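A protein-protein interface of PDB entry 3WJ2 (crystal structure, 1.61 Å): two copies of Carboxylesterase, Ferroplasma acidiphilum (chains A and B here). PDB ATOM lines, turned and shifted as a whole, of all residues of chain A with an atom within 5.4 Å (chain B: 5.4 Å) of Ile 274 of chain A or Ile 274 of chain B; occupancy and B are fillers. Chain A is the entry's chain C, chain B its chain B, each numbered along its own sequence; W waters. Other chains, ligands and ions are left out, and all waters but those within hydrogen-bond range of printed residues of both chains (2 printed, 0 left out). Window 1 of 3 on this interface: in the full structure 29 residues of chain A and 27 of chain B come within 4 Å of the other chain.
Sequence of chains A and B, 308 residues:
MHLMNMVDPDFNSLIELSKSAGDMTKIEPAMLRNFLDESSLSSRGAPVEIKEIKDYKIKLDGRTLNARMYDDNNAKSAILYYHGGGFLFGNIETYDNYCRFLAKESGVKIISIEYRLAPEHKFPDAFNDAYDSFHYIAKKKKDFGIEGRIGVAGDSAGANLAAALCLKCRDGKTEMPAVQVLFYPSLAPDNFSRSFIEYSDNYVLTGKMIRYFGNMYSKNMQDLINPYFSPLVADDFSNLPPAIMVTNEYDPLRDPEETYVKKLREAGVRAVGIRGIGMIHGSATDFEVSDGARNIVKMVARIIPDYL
The backbone NH (N) of Ile 277 of chain B is in hydrogen-bond range of the backbone carbonyl oxygen (O) of Gly 273 of chain A (2.8 Å). The backbone carbonyl oxygen of Gly 273 of chain B is in hydrogen-bond range of the backbone NH of Ile 277 of chain A. O of Arg 275 of chain B lies within hydrogen-bond range of N of Arg 275 of chain A (2.9 Å).
Among the printed residues, pairs that only touch across the chains: Val 272 of chain A with Ile 296 of chain B, Gly 273 of chain A with Arg 275 of chain B, Gly 273 of chain A with Gly 276 of chain B, Ile 274 of chain A with Ile 274 of chain B, Ile 274 of chain A with Arg 275 of chain B, Ile 274 of chain A with Ile 277 of chain B, Ile 274 of chain A with Ile 296 of chain B, Ile 274 of chain A with Met 299 of chain B, Arg 275 of chain A with Gly 273 of chain B, Arg 275 of chain A with Ile 274 of chain B, Gly 276 of chain A with Gly 273 of chain B, Ile 277 of chain A with Ile 274 of chain B, Ile 296 of chain A with Val 272 of chain B, Ile 296 of chain A with Ile 274 of chain B, Met 299 of chain A with Val 272 of chain B, Met 299 of chain A with Ile 274 of chain B, Met 299 of chain A with Met 299 of chain B and Val 300 of chain A with Met 299 of chain B.
N of Thr 247 of chain B sits at hydrogen-bond distance from O of Ile 274 of chain B, 2.9 Å away. The backbone NH (N) of Gly 276 of chain A is in hydrogen-bond range of the backbone carbonyl oxygen (O) of Thr 247 of chain A. The backbone NH (N) of Thr 247 of chain A sits at hydrogen-bond distance from the backbone carbonyl oxygen (O) of Ile 274 of chain A (2.8 Å). O of Met 245 of chain B sits at hydrogen-bond distance from N of Ile 274 of chain B. The backbone NH (N) of Met 245 of chain B sits at hydrogen-bond distance from the backbone carbonyl oxygen (O) of Val 272 of chain B (2.9 Å). O of Met 245 of chain A is in hydrogen-bond range of N of Ile 274 of chain A (2.9 Å).
Thr 247 of chain A touches none of the printed residues of chain B. Of chain B, only Ile 274, Arg 275, Ile 277, Ile 296 and Met 299 come within 4 Å of Ile 274 of chain A. Printed residues of chain B within 4 Å of Val 300 of chain A: Met 299. Of the printed residues of chain A, Gly 273 of chain B touches Arg 275 (3.8 Å), Gly 276 (3.7 Å) and Ile 277 (2.9 Å). Of the printed residues of chain A, Ile 274 of chain B touches Ile 274 (3.9 Å), Arg 275 (3.3 Å), Ile 277 (3.8 Å), Ile 296 (3.9995 Å) and Met 299 (3.9 Å). Printed residues of chain A within 4 Å of Arg 275 of chain B: Gly 273, Ile 274 and Arg 275. The nearest printed residue of chain A that does not touch Ile 274 of chain B is Gly 276 of chain A (4.6 Å). The nearest printed residue of chain A that does not touch Ile 277 of chain B is Arg 275 of chain A (4.1 Å).
Water W2 lies within hydrogen-bond range of N of Gly 273 of chain B (2.8 Å) and O of Ile 277 of chain A (2.9 Å). Water W1 bridges O of Ile 277 of chain B and N of Gly 273 of chain A.
Hydrophobic or aromatic side chains of chain B within 4 Å of the printed part of chain A: Val 272, Ile 274, Ile 277, Ile 296 and Met 299. Along chain B the printed residues that touch a printed residue of chain A span positions 272 to 299. Hydrophobic or aromatic side chains of chain A within 4 Å of the printed part of chain B: Val 272, Ile 274, Ile 277, Ile 296, Met 299 and Val 300. Along chain A the printed residues that touch a printed residue of chain B span positions 272 to 300. Among the printed residues, 21 pairs touch across the chains.
Ile 274 of chain A touches Arg 275 of chain B, and with the chains exchanged Arg 275 of chain A touches Ile 274 of chain B. Ile 274 of chain A touches Ile 277 of chain B, and with the chains exchanged Ile 277 of chain A touches Ile 274 of chain B. Ile 274 of chain A touches Met 299 of chain B, and with the chains exchanged Met 299 of chain A touches Ile 274 of chain B. Arg 275 of chain B touches its own counterpart, Arg 275 of chain A.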
ATOM      1  N   MET A 245      -0.973  25.257  28.262  1.00  0.00           N
ATOM      2  CA  MET A 245      -1.598  24.308  27.344  1.00  0.00           C
ATOM      3  C   MET A 245      -1.055  22.914  27.635  1.00  0.00           C
ATOM      4  O   MET A 245       0.196  22.738  27.600  1.00  0.00           O
ATOM      5  CB  MET A 245      -1.312  24.663  25.859  1.00  0.00           C
ATOM      6  CG  MET A 245      -1.842  23.638  24.826  1.00  0.00           C
ATOM      7  SD  MET A 245      -3.669  23.588  24.728  1.00  0.00           S
ATOM      8  CE  MET A 245      -3.916  24.983  23.649  1.00  0.00           C
ATOM      9  N   VAL A 246      -1.971  21.925  27.805  1.00  0.00           N
ATOM     10  CA  VAL A 246      -1.491  20.529  28.026  1.00  0.00           C
ATOM     11  C   VAL A 246      -2.121  19.736  26.861  1.00  0.00           C
ATOM     12  O   VAL A 246      -3.309  19.797  26.645  1.00  0.00           O
ATOM     13  CB  VAL A 246      -2.023  19.997  29.349  1.00  0.00           C
ATOM     14  CG1 VAL A 246      -1.691  18.450  29.442  1.00  0.00           C
ATOM     15  CG2 VAL A 246      -1.468  20.871  30.552  1.00  0.00           C
ATOM     16  N   THR A 247      -1.254  19.037  26.122  1.00  0.00           N
ATOM     17  CA  THR A 247      -1.779  18.147  25.063  1.00  0.00           C
ATOM     18  C   THR A 247      -1.408  16.770  25.446  1.00  0.00           C
ATOM     19  O   THR A 247      -0.546  16.508  26.288  1.00  0.00           O
ATOM     20  CB  THR A 247      -1.211  18.523  23.662  1.00  0.00           C
ATOM     21  OG1 THR A 247       0.149  18.096  23.577  1.00  0.00           O
ATOM     22  CG2 THR A 247      -1.359  20.062  23.517  1.00  0.00           C
ATOM     23  N   VAL A 272       2.981  28.514  27.931  1.00  0.00           N
ATOM     24  CA  VAL A 272       3.830  27.303  28.036  1.00  0.00           C
ATOM     25  C   VAL A 272       2.922  26.132  27.585  1.00  0.00           C
ATOM     26  O   VAL A 272       1.741  26.098  27.958  1.00  0.00           O
ATOM     27  CB  VAL A 272       4.348  27.106  29.491  1.00  0.00           C
ATOM     28  CG1 VAL A 272       3.235  27.084  30.553  1.00  0.00           C
ATOM     29  CG2 VAL A 272       5.283  25.819  29.551  1.00  0.00           C
ATOM     30  N   GLY A 273       3.492  25.282  26.746  1.00  0.00           N
ATOM     31  CA  GLY A 273       2.710  24.080  26.289  1.00  0.00           C
ATOM     32  C   GLY A 273       3.565  22.858  26.586  1.00  0.00           C
ATOM     33  O   GLY A 273       4.792  22.805  26.281  1.00  0.00           O
ATOM     34  N   ILE A 274       2.838  21.802  27.058  1.00  0.00           N
ATOM     35  CA  ILE A 274       3.551  20.528  27.236  1.00  0.00           C
ATOM     36  C   ILE A 274       2.663  19.450  26.620  1.00  0.00           C
ATOM     37  O   ILE A 274       1.435  19.467  26.774  1.00  0.00           O
ATOM     38  CB  ILE A 274       3.832  20.251  28.792  1.00  0.00           C
ATOM     39  CG1 ILE A 274       2.578  20.395  29.629  1.00  0.00           C
ATOM     40  CG2 ILE A 274       4.969  21.127  29.307  1.00  0.00           C
ATOM     41  CD1 ILE A 274       2.745  19.812  31.107  1.00  0.00           C
ATOM     42  N   ARG A 275       3.314  18.543  25.930  1.00  0.00           N
ATOM     43  CA  ARG A 275       2.658  17.282  25.459  1.00  0.00           C
ATOM     44  C   ARG A 275       3.021  16.176  26.393  1.00  0.00           C
ATOM     45  O   ARG A 275       4.172  15.840  26.622  1.00  0.00           O
ATOM     46  CB  ARG A 275       3.177  16.995  24.033  1.00  0.00           C
ATOM     47  CG  ARG A 275       2.593  15.590  23.510  1.00  0.00           C
ATOM     48  CD  ARG A 275       3.497  15.110  22.428  1.00  0.00           C
ATOM     49  NE  ARG A 275       3.273  15.832  21.189  1.00  0.00           N
ATOM     50  CZ  ARG A 275       3.568  15.406  19.957  1.00  0.00           C
ATOM     51  NH1 ARG A 275       3.209  16.152  18.888  1.00  0.00           N
ATOM     52  NH2 ARG A 275       4.220  14.221  19.787  1.00  0.00           N
ATOM     53  N   GLY A 276       1.969  15.472  26.869  1.00  0.00           N
ATOM     54  CA  GLY A 276       2.190  14.364  27.816  1.00  0.00           C
ATOM     55  C   GLY A 276       2.499  13.119  26.976  1.00  0.00           C
ATOM     56  O   GLY A 276       1.646  12.655  26.191  1.00  0.00           O
ATOM     57  N   ILE A 277       3.696  12.541  27.169  1.00  0.00           N
ATOM     58  CA  ILE A 277       4.192  11.403  26.369  1.00  0.00           C
ATOM     59  C   ILE A 277       3.414  10.146  26.834  1.00  0.00           C
ATOM     60  O   ILE A 277       3.292   9.855  28.027  1.00  0.00           O
ATOM     61  CB  ILE A 277       5.705  11.286  26.556  1.00  0.00           C
ATOM     62  CG1 ILE A 277       6.375  12.499  25.930  1.00  0.00           C
ATOM     63  CG2 ILE A 277       6.181   9.939  25.902  1.00  0.00           C
ATOM     64  CD1 ILE A 277       7.849  12.739  26.381  1.00  0.00           C
ATOM     65  N   ILE A 296       1.305  15.086  35.696  1.00  0.00           N
ATOM     66  CA  ILE A 296       1.104  16.214  34.753  1.00  0.00           C
ATOM     67  C   ILE A 296       0.109  17.203  35.411  1.00  0.00           C
ATOM     68  O   ILE A 296       0.334  18.428  35.392  1.00  0.00           O
ATOM     69  CB  ILE A 296       0.628  15.713  33.383  1.00  0.00           C
ATOM     70  CG1 ILE A 296       1.829  15.008  32.723  1.00  0.00           C
ATOM     71  CG2 ILE A 296       0.107  16.924  32.579  1.00  0.00           C
ATOM     72  CD1 ILE A 296       1.311  14.150  31.519  1.00  0.00           C
ATOM     73  N   MET A 299       1.886  19.049  38.159  1.00  0.00           N
ATOM     74  CA  MET A 299       2.840  20.019  37.617  1.00  0.00           C
ATOM     75  C   MET A 299       2.060  21.348  37.341  1.00  0.00           C
ATOM     76  O   MET A 299       2.523  22.428  37.705  1.00  0.00           O
ATOM     77  CB  MET A 299       3.531  19.520  36.328  1.00  0.00           C
ATOM     78  CG  MET A 299       4.663  18.476  36.557  1.00  0.00           C
ATOM     79  SD  MET A 299       4.956  18.012  34.712  1.00  0.00           S
ATOM     80  CE  MET A 299       5.405  16.330  34.875  1.00  0.00           C
ATOM     81  N   VAL A 300       0.997  21.196  36.582  1.00  0.00           N
ATOM     82  CA  VAL A 300       0.228  22.395  36.160  1.00  0.00           C
ATOM     83  C   VAL A 300      -0.394  23.111  37.405  1.00  0.00           C
ATOM     84  O   VAL A 300      -0.282  24.341  37.574  1.00  0.00           O
ATOM     85  CB  VAL A 300      -0.870  21.955  35.215  1.00  0.00           C
ATOM     86  CG1 VAL A 300      -1.837  23.200  34.965  1.00  0.00           C
ATOM     87  CG2 VAL A 300      -0.257  21.513  33.867  1.00  0.00           C
ATOM     88  N   MET B 245      10.889  12.776  32.819  1.00  0.00           N
ATOM     89  CA  MET B 245      11.627  12.976  31.561  1.00  0.00           C
ATOM     90  C   MET B 245      11.076  14.225  30.921  1.00  0.00           C
ATOM     91  O   MET B 245       9.873  14.376  30.770  1.00  0.00           O
ATOM     92  CB  MET B 245      11.450  11.824  30.543  1.00  0.00           C
ATOM     93  CG  MET B 245      12.049  12.132  29.185  1.00  0.00           C
ATOM     94  SD  MET B 245      13.880  11.999  29.203  1.00  0.00           S
ATOM     95  CE  MET B 245      14.132  10.159  29.222  1.00  0.00           C
ATOM     96  N   VAL B 246      12.010  15.154  30.611  1.00  0.00           N
ATOM     97  CA  VAL B 246      11.577  16.376  29.858  1.00  0.00           C
ATOM     98  C   VAL B 246      12.330  16.343  28.560  1.00  0.00           C
ATOM     99  O   VAL B 246      13.542  16.252  28.481  1.00  0.00           O
ATOM    100  CB  VAL B 246      12.052  17.636  30.662  1.00  0.00           C
ATOM    101  CG1 VAL B 246      11.679  18.899  29.860  1.00  0.00           C
ATOM    102  CG2 VAL B 246      11.356  17.621  32.095  1.00  0.00           C
ATOM    103  N   THR B 247      11.580  16.437  27.461  1.00  0.00           N
ATOM    104  CA  THR B 247      12.192  16.570  26.130  1.00  0.00           C
ATOM    105  C   THR B 247      11.718  17.897  25.536  1.00  0.00           C
ATOM    106  O   THR B 247      10.832  18.588  26.059  1.00  0.00           O
ATOM    107  CB  THR B 247      11.639  15.406  25.175  1.00  0.00           C
ATOM    108  OG1 THR B 247      10.283  15.696  24.837  1.00  0.00           O
ATOM    109  CG2 THR B 247      11.679  14.088  25.958  1.00  0.00           C
ATOM    110  N   VAL B 272       6.867   9.850  34.208  1.00  0.00           N
ATOM    111  CA  VAL B 272       6.098  10.902  33.517  1.00  0.00           C
ATOM    112  C   VAL B 272       6.999  11.548  32.536  1.00  0.00           C
ATOM    113  O   VAL B 272       8.179  11.811  32.854  1.00  0.00           O
ATOM    114  CB  VAL B 272       5.493  11.876  34.600  1.00  0.00           C
ATOM    115  CG1 VAL B 272       6.564  12.537  35.564  1.00  0.00           C
ATOM    116  CG2 VAL B 272       4.666  12.959  33.833  1.00  0.00           C
ATOM    117  N   GLY B 273       6.504  11.719  31.315  1.00  0.00           N
ATOM    118  CA  GLY B 273       7.309  12.349  30.287  1.00  0.00           C
ATOM    119  C   GLY B 273       6.545  13.534  29.711  1.00  0.00           C
ATOM    120  O   GLY B 273       5.367  13.384  29.323  1.00  0.00           O
ATOM    121  N   ILE B 274       7.250  14.691  29.585  1.00  0.00           N
ATOM    122  CA  ILE B 274       6.601  15.869  28.920  1.00  0.00           C
ATOM    123  C   ILE B 274       7.514  16.399  27.855  1.00  0.00           C
ATOM    124  O   ILE B 274       8.726  16.450  28.083  1.00  0.00           O
ATOM    125  CB  ILE B 274       6.196  16.997  29.920  1.00  0.00           C
ATOM    126  CG1 ILE B 274       7.394  17.330  30.795  1.00  0.00           C
ATOM    127  CG2 ILE B 274       4.954  16.570  30.776  1.00  0.00           C
ATOM    128  CD1 ILE B 274       7.185  18.656  31.591  1.00  0.00           C
ATOM    129  N   ARG B 275       6.948  16.748  26.673  1.00  0.00           N
ATOM    130  CA  ARG B 275       7.688  17.454  25.608  1.00  0.00           C
ATOM    131  C   ARG B 275       7.304  18.905  25.640  1.00  0.00           C
ATOM    132  O   ARG B 275       6.106  19.214  25.649  1.00  0.00           O
ATOM    133  CB  ARG B 275       7.289  16.871  24.238  1.00  0.00           C
ATOM    134  CG  ARG B 275       7.894  17.653  23.082  1.00  0.00           C
ATOM    135  CD  ARG B 275       7.116  17.367  21.750  1.00  0.00           C
ATOM    136  NE  ARG B 275       7.424  16.004  21.270  1.00  0.00           N
ATOM    137  CZ  ARG B 275       7.217  15.698  19.975  1.00  0.00           C
ATOM    138  NH1 ARG B 275       6.572  16.586  19.136  1.00  0.00           N
ATOM    139  NH2 ARG B 275       7.657  14.473  19.578  1.00  0.00           N
ATOM    140  N   GLY B 276       8.347  19.745  25.760  1.00  0.00           N
ATOM    141  CA  GLY B 276       8.027  21.219  25.783  1.00  0.00           C
ATOM    142  C   GLY B 276       7.802  21.713  24.378  1.00  0.00           C
ATOM    143  O   GLY B 276       8.726  21.612  23.530  1.00  0.00           O
ATOM    144  N   ILE B 277       6.588  22.250  24.170  1.00  0.00           N
ATOM    145  CA  ILE B 277       6.198  22.712  22.808  1.00  0.00           C
ATOM    146  C   ILE B 277       6.993  23.994  22.508  1.00  0.00           C
ATOM    147  O   ILE B 277       7.063  24.910  23.336  1.00  0.00           O
ATOM    148  CB  ILE B 277       4.709  22.880  22.775  1.00  0.00           C
ATOM    149  CG1 ILE B 277       4.072  21.464  22.823  1.00  0.00           C
ATOM    150  CG2 ILE B 277       4.285  23.524  21.385  1.00  0.00           C
ATOM    151  CD1 ILE B 277       2.600  21.550  23.298  1.00  0.00           C
ATOM    152  N   ILE B 296       8.388  25.295  32.651  1.00  0.00           N
ATOM    153  CA  ILE B 296       8.641  23.788  32.602  1.00  0.00           C
ATOM    154  C   ILE B 296       9.558  23.405  33.721  1.00  0.00           C
ATOM    155  O   ILE B 296       9.294  22.384  34.424  1.00  0.00           O
ATOM    156  CB  ILE B 296       9.138  23.381  31.197  1.00  0.00           C
ATOM    157  CG1 ILE B 296       7.977  23.505  30.247  1.00  0.00           C
ATOM    158  CG2 ILE B 296       9.808  21.942  31.180  1.00  0.00           C
ATOM    159  CD1 ILE B 296       8.477  23.483  28.770  1.00  0.00           C
ATOM    160  N   MET B 299       7.604  23.518  36.960  1.00  0.00           N
ATOM    161  CA  MET B 299       6.649  22.389  36.984  1.00  0.00           C
ATOM    162  C   MET B 299       7.425  21.175  37.582  1.00  0.00           C
ATOM    163  O   MET B 299       6.921  20.509  38.486  1.00  0.00           O
ATOM    164  CB  MET B 299       6.147  22.054  35.551  1.00  0.00           C
ATOM    165  CG  MET B 299       5.010  22.877  35.230  1.00  0.00           C
ATOM    166  SD  MET B 299       4.758  22.353  33.399  1.00  0.00           S
ATOM    167  CE  MET B 299       3.245  22.969  33.771  1.00  0.00           C
ATOM    168  N   VAL B 300       8.547  20.871  37.032  1.00  0.00           N
ATOM    169  CA  VAL B 300       9.330  19.703  37.458  1.00  0.00           C
ATOM    170  C   VAL B 300       9.806  19.891  38.885  1.00  0.00           C
ATOM    171  O   VAL B 300       9.634  19.014  39.739  1.00  0.00           O
ATOM    172  CB  VAL B 300      10.482  19.471  36.489  1.00  0.00           C
ATOM    173  CG1 VAL B 300      11.378  18.384  37.049  1.00  0.00           C
ATOM    174  CG2 VAL B 300       9.898  19.022  35.098  1.00  0.00           C
HETATM  175  O   HOH W   1       6.137  25.853  25.828  1.00  0.00           O
HETATM  176  O   HOH W   2       3.952  10.691  30.711  1.00  0.00           O
